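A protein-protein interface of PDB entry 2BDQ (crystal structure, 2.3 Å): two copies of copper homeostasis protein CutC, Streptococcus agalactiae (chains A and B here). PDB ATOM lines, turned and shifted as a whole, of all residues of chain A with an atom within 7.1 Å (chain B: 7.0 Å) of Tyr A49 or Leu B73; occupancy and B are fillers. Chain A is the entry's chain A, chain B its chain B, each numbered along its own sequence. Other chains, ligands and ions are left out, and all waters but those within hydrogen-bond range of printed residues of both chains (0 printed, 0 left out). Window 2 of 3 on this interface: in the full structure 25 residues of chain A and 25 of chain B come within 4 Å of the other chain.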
ATOM      1  N   LEU A  11      21.264  27.676 -14.882  1.00  0.00           N
ATOM      2  CA  LEU A  11      20.467  27.879 -16.085  1.00  0.00           C
ATOM      3  C   LEU A  11      19.063  27.337 -16.084  1.00  0.00           C
ATOM      4  O   LEU A  11      18.447  27.165 -17.130  1.00  0.00           O
ATOM      5  CB  LEU A  11      21.238  27.387 -17.309  1.00  0.00           C
ATOM      6  CG  LEU A  11      21.956  26.050 -17.249  1.00  0.00           C
ATOM      7  CD1 LEU A  11      20.981  24.933 -17.604  1.00  0.00           C
ATOM      8  CD2 LEU A  11      23.123  26.074 -18.228  1.00  0.00           C
ATOM      9  N   ASP A  13      16.209  28.784 -15.126  1.00  0.00           N
ATOM     10  CA  ASP A  13      15.200  29.702 -15.640  1.00  0.00           C
ATOM     11  C   ASP A  13      15.557  30.376 -16.957  1.00  0.00           C
ATOM     12  O   ASP A  13      14.893  31.326 -17.362  1.00  0.00           O
ATOM     13  CB  ASP A  13      14.917  30.766 -14.580  1.00  0.00           C
ATOM     14  CG  ASP A  13      14.578  30.161 -13.233  1.00  0.00           C
ATOM     15  OD1 ASP A  13      14.977  30.739 -12.200  1.00  0.00           O
ATOM     16  OD2 ASP A  13      13.911  29.106 -13.205  1.00  0.00           O
ATOM     17  N   LEU A  14      16.582  29.880 -17.636  1.00  0.00           N
ATOM     18  CA  LEU A  14      16.999  30.491 -18.893  1.00  0.00           C
ATOM     19  C   LEU A  14      16.174  30.101 -20.117  1.00  0.00           C
ATOM     20  O   LEU A  14      16.146  30.836 -21.102  1.00  0.00           O
ATOM     21  CB  LEU A  14      18.473  30.183 -19.171  1.00  0.00           C
ATOM     22  CG  LEU A  14      19.525  30.702 -18.189  1.00  0.00           C
ATOM     23  CD1 LEU A  14      20.888  30.362 -18.751  1.00  0.00           C
ATOM     24  CD2 LEU A  14      19.396  32.204 -17.979  1.00  0.00           C
ATOM     25  N   THR A  15      15.490  28.964 -20.050  1.00  0.00           N
ATOM     26  CA  THR A  15      14.706  28.488 -21.184  1.00  0.00           C
ATOM     27  C   THR A  15      13.570  29.397 -21.636  1.00  0.00           C
ATOM     28  O   THR A  15      13.068  29.251 -22.747  1.00  0.00           O
ATOM     29  CB  THR A  15      14.141  27.072 -20.916  1.00  0.00           C
ATOM     30  OG1 THR A  15      13.573  27.016 -19.602  1.00  0.00           O
ATOM     31  CG2 THR A  15      15.249  26.033 -21.031  1.00  0.00           C
ATOM     32  N   ARG A  16      13.171  30.350 -20.801  1.00  0.00           N
ATOM     33  CA  ARG A  16      12.083  31.244 -21.186  1.00  0.00           C
ATOM     34  C   ARG A  16      12.567  32.623 -21.634  1.00  0.00           C
ATOM     35  O   ARG A  16      11.766  33.470 -22.028  1.00  0.00           O
ATOM     36  CB  ARG A  16      11.092  31.403 -20.029  1.00  0.00           C
ATOM     37  CG  ARG A  16       9.656  31.626 -20.487  1.00  0.00           C
ATOM     38  CD  ARG A  16       9.182  30.441 -21.329  1.00  0.00           C
ATOM     39  NE  ARG A  16       9.286  29.189 -20.580  1.00  0.00           N
ATOM     40  CZ  ARG A  16       9.548  28.004 -21.123  1.00  0.00           C
ATOM     41  NH1 ARG A  16       9.622  26.922 -20.354  1.00  0.00           N
ATOM     42  NH2 ARG A  16       9.746  27.902 -22.432  1.00  0.00           N
ATOM     43  N   LEU A  17      13.876  32.850 -21.580  1.00  0.00           N
ATOM     44  CA  LEU A  17      14.421  34.140 -21.983  1.00  0.00           C
ATOM     45  C   LEU A  17      14.336  34.357 -23.485  1.00  0.00           C
ATOM     46  O   LEU A  17      14.485  33.421 -24.271  1.00  0.00           O
ATOM     47  CB  LEU A  17      15.876  34.280 -21.524  1.00  0.00           C
ATOM     48  CG  LEU A  17      16.146  34.769 -20.097  1.00  0.00           C
ATOM     49  CD1 LEU A  17      15.365  33.942 -19.095  1.00  0.00           C
ATOM     50  CD2 LEU A  17      17.635  34.688 -19.811  1.00  0.00           C
ATOM     51  N   GLY A  41      31.009  24.024 -15.300  1.00  0.00           N
ATOM     52  CA  GLY A  41      30.030  23.465 -16.213  1.00  0.00           C
ATOM     53  C   GLY A  41      28.900  24.429 -16.527  1.00  0.00           C
ATOM     54  O   GLY A  41      28.460  24.523 -17.674  1.00  0.00           O
ATOM     55  N   ILE A  43      28.988  27.746 -16.411  1.00  0.00           N
ATOM     56  CA  ILE A  43      29.493  28.852 -17.232  1.00  0.00           C
ATOM     57  C   ILE A  43      29.624  28.440 -18.706  1.00  0.00           C
ATOM     58  O   ILE A  43      29.160  29.145 -19.610  1.00  0.00           O
ATOM     59  CB  ILE A  43      30.872  29.347 -16.709  1.00  0.00           C
ATOM     60  CG1 ILE A  43      30.713  29.935 -15.300  1.00  0.00           C
ATOM     61  CG2 ILE A  43      31.439  30.418 -17.639  1.00  0.00           C
ATOM     62  CD1 ILE A  43      32.035  30.324 -14.640  1.00  0.00           C
ATOM     63  N   LYS A  44      30.246  27.294 -18.945  1.00  0.00           N
ATOM     64  CA  LYS A  44      30.441  26.802 -20.304  1.00  0.00           C
ATOM     65  C   LYS A  44      29.123  26.571 -21.039  1.00  0.00           C
ATOM     66  O   LYS A  44      28.931  27.053 -22.160  1.00  0.00           O
ATOM     67  CB  LYS A  44      31.242  25.503 -20.275  1.00  0.00           C
ATOM     68  CG  LYS A  44      31.366  24.775 -21.611  1.00  0.00           C
ATOM     69  CD  LYS A  44      32.163  23.484 -21.414  1.00  0.00           C
ATOM     70  CE  LYS A  44      32.198  22.617 -22.662  1.00  0.00           C
ATOM     71  NZ  LYS A  44      32.842  23.320 -23.801  1.00  0.00           N
ATOM     72  N   GLU A  45      28.216  25.833 -20.411  1.00  0.00           N
ATOM     73  CA  GLU A  45      26.935  25.540 -21.036  1.00  0.00           C
ATOM     74  C   GLU A  45      26.002  26.739 -21.135  1.00  0.00           C
ATOM     75  O   GLU A  45      25.305  26.902 -22.132  1.00  0.00           O
ATOM     76  CB  GLU A  45      26.247  24.394 -20.293  1.00  0.00           C
ATOM     77  CG  GLU A  45      27.042  23.087 -20.319  1.00  0.00           C
ATOM     78  CD  GLU A  45      27.438  22.675 -21.733  1.00  0.00           C
ATOM     79  OE1 GLU A  45      26.562  22.692 -22.629  1.00  0.00           O
ATOM     80  OE2 GLU A  45      28.620  22.325 -21.948  1.00  0.00           O
ATOM     81  N   ALA A  46      25.979  27.571 -20.101  1.00  0.00           N
ATOM     82  CA  ALA A  46      25.123  28.744 -20.118  1.00  0.00           C
ATOM     83  C   ALA A  46      25.556  29.681 -21.246  1.00  0.00           C
ATOM     84  O   ALA A  46      24.720  30.153 -22.014  1.00  0.00           O
ATOM     85  CB  ALA A  46      25.181  29.464 -18.780  1.00  0.00           C
ATOM     86  N   ASN A  47      26.858  29.936 -21.352  1.00  0.00           N
ATOM     87  CA  ASN A  47      27.371  30.819 -22.399  1.00  0.00           C
ATOM     88  C   ASN A  47      26.991  30.336 -23.792  1.00  0.00           C
ATOM     89  O   ASN A  47      26.568  31.121 -24.637  1.00  0.00           O
ATOM     90  CB  ASN A  47      28.894  30.943 -22.316  1.00  0.00           C
ATOM     91  CG  ASN A  47      29.350  31.733 -21.109  1.00  0.00           C
ATOM     92  OD1 ASN A  47      30.548  31.931 -20.898  1.00  0.00           O
ATOM     93  ND2 ASN A  47      28.399  32.184 -20.300  1.00  0.00           N
ATOM     94  N   GLN A  48      27.148  29.040 -24.034  1.00  0.00           N
ATOM     95  CA  GLN A  48      26.812  28.473 -25.334  1.00  0.00           C
ATOM     96  C   GLN A  48      25.307  28.518 -25.563  1.00  0.00           C
ATOM     97  O   GLN A  48      24.855  28.823 -26.661  1.00  0.00           O
ATOM     98  CB  GLN A  48      27.312  27.030 -25.422  1.00  0.00           C
ATOM     99  CG  GLN A  48      27.048  26.346 -26.757  1.00  0.00           C
ATOM    100  CD  GLN A  48      27.707  24.976 -26.834  1.00  0.00           C
ATOM    101  OE1 GLN A  48      28.901  24.832 -26.545  1.00  0.00           O
ATOM    102  NE2 GLN A  48      26.937  23.965 -27.228  1.00  0.00           N
ATOM    103  N   TYR A  49      24.539  28.221 -24.521  1.00  0.00           N
ATOM    104  CA  TYR A  49      23.084  28.230 -24.616  1.00  0.00           C
ATOM    105  C   TYR A  49      22.558  29.637 -24.871  1.00  0.00           C
ATOM    106  O   TYR A  49      21.736  29.846 -25.756  1.00  0.00           O
ATOM    107  CB  TYR A  49      22.462  27.694 -23.328  1.00  0.00           C
ATOM    108  CG  TYR A  49      20.954  27.615 -23.364  1.00  0.00           C
ATOM    109  CD1 TYR A  49      20.307  26.563 -24.004  1.00  0.00           C
ATOM    110  CD2 TYR A  49      20.173  28.598 -22.755  1.00  0.00           C
ATOM    111  CE1 TYR A  49      18.909  26.487 -24.035  1.00  0.00           C
ATOM    112  CE2 TYR A  49      18.783  28.534 -22.781  1.00  0.00           C
ATOM    113  CZ  TYR A  49      18.157  27.473 -23.420  1.00  0.00           C
ATOM    114  OH  TYR A  49      16.783  27.393 -23.436  1.00  0.00           O
ATOM    115  N   LEU A  50      23.031  30.601 -24.089  1.00  0.00           N
ATOM    116  CA  LEU A  50      22.590  31.978 -24.245  1.00  0.00           C
ATOM    117  C   LEU A  50      23.079  32.603 -25.550  1.00  0.00           C
ATOM    118  O   LEU A  50      22.316  33.283 -26.231  1.00  0.00           O
ATOM    119  CB  LEU A  50      23.047  32.813 -23.052  1.00  0.00           C
ATOM    120  CG  LEU A  50      22.399  32.427 -21.718  1.00  0.00           C
ATOM    121  CD1 LEU A  50      23.137  33.111 -20.587  1.00  0.00           C
ATOM    122  CD2 LEU A  50      20.913  32.801 -21.719  1.00  0.00           C
ATOM    123  N   HIS A  51      24.342  32.382 -25.904  1.00  0.00           N
ATOM    124  CA  HIS A  51      24.866  32.935 -27.148  1.00  0.00           C
ATOM    125  C   HIS A  51      24.040  32.409 -28.314  1.00  0.00           C
ATOM    126  O   HIS A  51      23.770  33.128 -29.273  1.00  0.00           O
ATOM    127  CB  HIS A  51      26.332  32.543 -27.339  1.00  0.00           C
ATOM    128  CG  HIS A  51      27.276  33.267 -26.431  1.00  0.00           C
ATOM    129  ND1 HIS A  51      28.597  32.902 -26.288  1.00  0.00           N
ATOM    130  CD2 HIS A  51      27.091  34.334 -25.617  1.00  0.00           C
ATOM    131  CE1 HIS A  51      29.185  33.709 -25.426  1.00  0.00           C
ATOM    132  NE2 HIS A  51      28.293  34.587 -25.004  1.00  0.00           N
ATOM    133  N   GLU A  52      23.635  31.149 -28.217  1.00  0.00           N
ATOM    134  CA  GLU A  52      22.831  30.516 -29.252  1.00  0.00           C
ATOM    135  C   GLU A  52      21.498  31.261 -29.414  1.00  0.00           C
ATOM    136  O   GLU A  52      20.977  31.362 -30.525  1.00  0.00           O
ATOM    137  CB  GLU A  52      22.602  29.053 -28.871  1.00  0.00           C
ATOM    138  CG  GLU A  52      21.942  28.169 -29.913  1.00  0.00           C
ATOM    139  CD  GLU A  52      22.053  26.688 -29.546  1.00  0.00           C
ATOM    140  OE1 GLU A  52      23.186  26.152 -29.606  1.00  0.00           O
ATOM    141  OE2 GLU A  52      21.021  26.066 -29.183  1.00  0.00           O
ATOM    142  N   LYS A  53      20.962  31.796 -28.315  1.00  0.00           N
ATOM    143  CA  LYS A  53      19.702  32.543 -28.353  1.00  0.00           C
ATOM    144  C   LYS A  53      19.960  34.038 -28.543  1.00  0.00           C
ATOM    145  O   LYS A  53      19.049  34.860 -28.444  1.00  0.00           O
ATOM    146  CB  LYS A  53      18.901  32.320 -27.065  1.00  0.00           C
ATOM    147  CG  LYS A  53      18.466  30.884 -26.851  1.00  0.00           C
ATOM    148  CD  LYS A  53      17.793  30.677 -25.501  1.00  0.00           C
ATOM    149  CE  LYS A  53      16.412  31.290 -25.432  1.00  0.00           C
ATOM    150  NZ  LYS A  53      15.777  30.974 -24.124  1.00  0.00           N
ATOM    151  N   GLY A  54      21.216  34.382 -28.811  1.00  0.00           N
ATOM    152  CA  GLY A  54      21.577  35.774 -29.025  1.00  0.00           C
ATOM    153  C   GLY A  54      21.527  36.685 -27.811  1.00  0.00           C
ATOM    154  O   GLY A  54      21.063  37.821 -27.895  1.00  0.00           O
ATOM    155  N   ILE A  55      21.998  36.199 -26.672  1.00  0.00           N
ATOM    156  CA  ILE A  55      22.000  37.028 -25.476  1.00  0.00           C
ATOM    157  C   ILE A  55      23.375  36.986 -24.812  1.00  0.00           C
ATOM    158  O   ILE A  55      24.004  35.930 -24.728  1.00  0.00           O
ATOM    159  CB  ILE A  55      20.897  36.583 -24.491  1.00  0.00           C
ATOM    160  CG1 ILE A  55      21.095  37.262 -23.142  1.00  0.00           C
ATOM    161  CG2 ILE A  55      20.900  35.078 -24.357  1.00  0.00           C
ATOM    162  CD1 ILE A  55      20.011  36.952 -22.146  1.00  0.00           C
ATOM    163  N   VAL A  57      26.303  37.379 -21.820  1.00  0.00           N
ATOM    164  CA  VAL A  57      26.458  36.798 -20.494  1.00  0.00           C
ATOM    165  C   VAL A  57      27.519  37.470 -19.641  1.00  0.00           C
ATOM    166  O   VAL A  57      28.681  37.491 -20.013  1.00  0.00           O
ATOM    167  CB  VAL A  57      26.847  35.315 -20.607  1.00  0.00           C
ATOM    168  CG1 VAL A  57      26.863  34.669 -19.224  1.00  0.00           C
ATOM    169  CG2 VAL A  57      25.889  34.600 -21.539  1.00  0.00           C
ATOM    170  N   PRO B  63      24.053  20.349 -10.498  1.00  0.00           N
ATOM    171  CA  PRO B  63      23.832  21.496 -11.388  1.00  0.00           C
ATOM    172  C   PRO B  63      22.874  22.576 -10.896  1.00  0.00           C
ATOM    173  O   PRO B  63      22.833  23.671 -11.464  1.00  0.00           O
ATOM    174  CB  PRO B  63      23.341  20.831 -12.665  1.00  0.00           C
ATOM    175  CG  PRO B  63      22.478  19.739 -12.122  1.00  0.00           C
ATOM    176  CD  PRO B  63      23.359  19.157 -11.024  1.00  0.00           C
ATOM    177  N   TYR B  70      17.327  15.095 -13.587  1.00  0.00           N
ATOM    178  CA  TYR B  70      18.007  16.010 -14.490  1.00  0.00           C
ATOM    179  C   TYR B  70      17.767  15.775 -15.970  1.00  0.00           C
ATOM    180  O   TYR B  70      17.656  14.636 -16.427  1.00  0.00           O
ATOM    181  CB  TYR B  70      19.518  15.976 -14.227  1.00  0.00           C
ATOM    182  CG  TYR B  70      19.893  16.212 -12.789  1.00  0.00           C
ATOM    183  CD1 TYR B  70      20.394  15.173 -11.992  1.00  0.00           C
ATOM    184  CD2 TYR B  70      19.731  17.472 -12.204  1.00  0.00           C
ATOM    185  CE1 TYR B  70      20.719  15.396 -10.651  1.00  0.00           C
ATOM    186  CE2 TYR B  70      20.053  17.690 -10.872  1.00  0.00           C
ATOM    187  CZ  TYR B  70      20.542  16.662 -10.103  1.00  0.00           C
ATOM    188  OH  TYR B  70      20.843  16.921  -8.780  1.00  0.00           O
ATOM    189  N   ASN B  71      17.699  16.874 -16.714  1.00  0.00           N
ATOM    190  CA  ASN B  71      17.500  16.805 -18.151  1.00  0.00           C
ATOM    191  C   ASN B  71      18.869  16.669 -18.807  1.00  0.00           C
ATOM    192  O   ASN B  71      19.900  16.800 -18.140  1.00  0.00           O
ATOM    193  CB  ASN B  71      16.752  18.054 -18.653  1.00  0.00           C
ATOM    194  CG  ASN B  71      17.508  19.345 -18.402  1.00  0.00           C
ATOM    195  OD1 ASN B  71      16.907  20.415 -18.310  1.00  0.00           O
ATOM    196  ND2 ASN B  71      18.826  19.260 -18.303  1.00  0.00           N
ATOM    197  N   ASP B  72      18.877  16.407 -20.108  1.00  0.00           N
ATOM    198  CA  ASP B  72      20.120  16.222 -20.858  1.00  0.00           C
ATOM    199  C   ASP B  72      21.168  17.309 -20.656  1.00  0.00           C
ATOM    200  O   ASP B  72      22.344  17.010 -20.433  1.00  0.00           O
ATOM    201  CB  ASP B  72      19.798  16.079 -22.350  1.00  0.00           C
ATOM    202  CG  ASP B  72      19.055  14.786 -22.656  1.00  0.00           C
ATOM    203  OD1 ASP B  72      18.503  14.648 -23.770  1.00  0.00           O
ATOM    204  OD2 ASP B  72      19.030  13.899 -21.773  1.00  0.00           O
ATOM    205  N   LEU B  73      20.741  18.566 -20.721  1.00  0.00           N
ATOM    206  CA  LEU B  73      21.650  19.694 -20.568  1.00  0.00           C
ATOM    207  C   LEU B  73      22.286  19.723 -19.171  1.00  0.00           C
ATOM    208  O   LEU B  73      23.471  20.023 -19.028  1.00  0.00           O
ATOM    209  CB  LEU B  73      20.893  20.992 -20.859  1.00  0.00           C
ATOM    210  CG  LEU B  73      21.733  22.207 -21.250  1.00  0.00           C
ATOM    211  CD1 LEU B  73      20.857  23.302 -21.864  1.00  0.00           C
ATOM    212  CD2 LEU B  73      22.454  22.716 -20.023  1.00  0.00           C
ATOM    213  N   GLU B  74      21.500  19.399 -18.151  1.00  0.00           N
ATOM    214  CA  GLU B  74      21.992  19.370 -16.786  1.00  0.00           C
ATOM    215  C   GLU B  74      22.969  18.210 -16.613  1.00  0.00           C
ATOM    216  O   GLU B  74      23.926  18.308 -15.846  1.00  0.00           O
ATOM    217  CB  GLU B  74      20.810  19.273 -15.814  1.00  0.00           C
ATOM    218  CG  GLU B  74      20.098  20.606 -15.641  1.00  0.00           C
ATOM    219  CD  GLU B  74      18.670  20.497 -15.143  1.00  0.00           C
ATOM    220  OE1 GLU B  74      18.071  21.563 -14.858  1.00  0.00           O
ATOM    221  OE2 GLU B  74      18.146  19.362 -15.049  1.00  0.00           O
ATOM    222  N   LEU B  75      22.738  17.114 -17.331  1.00  0.00           N
ATOM    223  CA  LEU B  75      23.646  15.974 -17.248  1.00  0.00           C
ATOM    224  C   LEU B  75      24.958  16.358 -17.935  1.00  0.00           C
ATOM    225  O   LEU B  75      26.026  15.921 -17.527  1.00  0.00           O
ATOM    226  CB  LEU B  75      23.033  14.729 -17.915  1.00  0.00           C
ATOM    227  CG  LEU B  75      21.833  14.091 -17.200  1.00  0.00           C
ATOM    228  CD1 LEU B  75      21.197  13.029 -18.093  1.00  0.00           C
ATOM    229  CD2 LEU B  75      22.283  13.480 -15.880  1.00  0.00           C
ATOM    230  N   ARG B  76      24.867  17.192 -18.966  1.00  0.00           N
ATOM    231  CA  ARG B  76      26.046  17.655 -19.696  1.00  0.00           C
ATOM    232  C   ARG B  76      26.870  18.550 -18.773  1.00  0.00           C
ATOM    233  O   ARG B  76      28.103  18.554 -18.824  1.00  0.00           O
ATOM    234  CB  ARG B  76      25.616  18.441 -20.940  1.00  0.00           C
ATOM    235  CG  ARG B  76      26.731  19.207 -21.670  1.00  0.00           C
ATOM    236  CD  ARG B  76      27.597  18.323 -22.566  1.00  0.00           C
ATOM    237  NE  ARG B  76      28.726  17.712 -21.861  1.00  0.00           N
ATOM    238  CZ  ARG B  76      29.804  18.372 -21.446  1.00  0.00           C
ATOM    239  NH1 ARG B  76      29.918  19.678 -21.657  1.00  0.00           N
ATOM    240  NH2 ARG B  76      30.780  17.720 -20.828  1.00  0.00           N
ATOM    241  N   ILE B  77      26.179  19.314 -17.933  1.00  0.00           N
ATOM    242  CA  ILE B  77      26.838  20.196 -16.984  1.00  0.00           C
ATOM    243  C   ILE B  77      27.611  19.350 -15.965  1.00  0.00           C
ATOM    244  O   ILE B  77      28.801  19.572 -15.727  1.00  0.00           O
ATOM    245  CB  ILE B  77      25.794  21.077 -16.262  1.00  0.00           C
ATOM    246  CG1 ILE B  77      25.272  22.141 -17.233  1.00  0.00           C
ATOM    247  CG2 ILE B  77      26.400  21.724 -15.022  1.00  0.00           C
ATOM    248  CD1 ILE B  77      24.051  22.882 -16.735  1.00  0.00           C
ATOM    249  N   MET B  78      26.925  18.371 -15.381  1.00  0.00           N
ATOM    250  CA  MET B  78      27.523  17.481 -14.388  1.00  0.00           C
ATOM    251  C   MET B  78      28.736  16.721 -14.929  1.00  0.00           C
ATOM    252  O   MET B  78      29.721  16.556 -14.218  1.00  0.00           O
ATOM    253  CB  MET B  78      26.468  16.499 -13.874  1.00  0.00           C
ATOM    254  CG  MET B  78      25.319  17.193 -13.150  1.00  0.00           C
ATOM    255  SD  MET B  78      23.836  16.019 -12.707  1.00  0.00           S
ATOM    256  CE  MET B  78      24.683  14.949 -11.349  1.00  0.00           C
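The side-chain carboxylate (OE2) of Glu A45 lies within salt-bridge range of the guanidinium group (NH1) of Arg B76 (3.0 Å).
N of Leu B73 sits close to ND2 of Asn B71 (3.2 Å).
Leu B73 touches Leu A11. Leu A11 touches Ile B77 (CD2 to CD1, 3.6 Å). C of Gly A41 touches CG2 of Ile B77, at 3.98 Å. CE of Lys A44 touches NH1 of Arg B76, 3.9 Å away. Ile B77 touches Glu A45. Tyr A49 touches Leu B73.
Of the printed residues of chain B, Leu A11 touches Leu B73 (3.6 Å) and Ile B77 (3.6 Å). Printed residues of chain B within 4 Å of Gly A41: Ile B77. Of the printed residues of chain B, Glu A45 touches Arg B76 (3.0 Å) and Ile B77 (3.7 Å). Ala A46 touches none of the printed residues of chain B. Of chain B, only Leu B73 comes within 4 Å of Tyr A49. Of chain A, only Leu A11 (3.6 Å) and Tyr A49 (3.9 Å) come within 4 Å of Leu B73. Printed residues of chain A within 4 Å of Arg B76: Lys A44 and Glu A45. The nearest printed residue of chain B that does not touch Tyr A49 is Ile B77 (8.3 Å). The nearest residue of chain A that does not touch Leu B73 is Glu A45 (4.2 Å). The nearest printed residue of chain B that does not touch Lys A44 is Ile B77 (7.0 Å).
Of the 21 printed residues of chain A, 5 touch a printed residue of chain B. Hydrophobic or aromatic side chains of chain A that line the printed part of chain B: Leu A11 and Tyr A49. Along chain B the printed residues that touch a printed residue of chain A span positions 73 to 77.
No position is printed for both chains. Of the 7 pairs that touch across the chains among the printed residues, none has its exchanged pair printed and touching as well.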
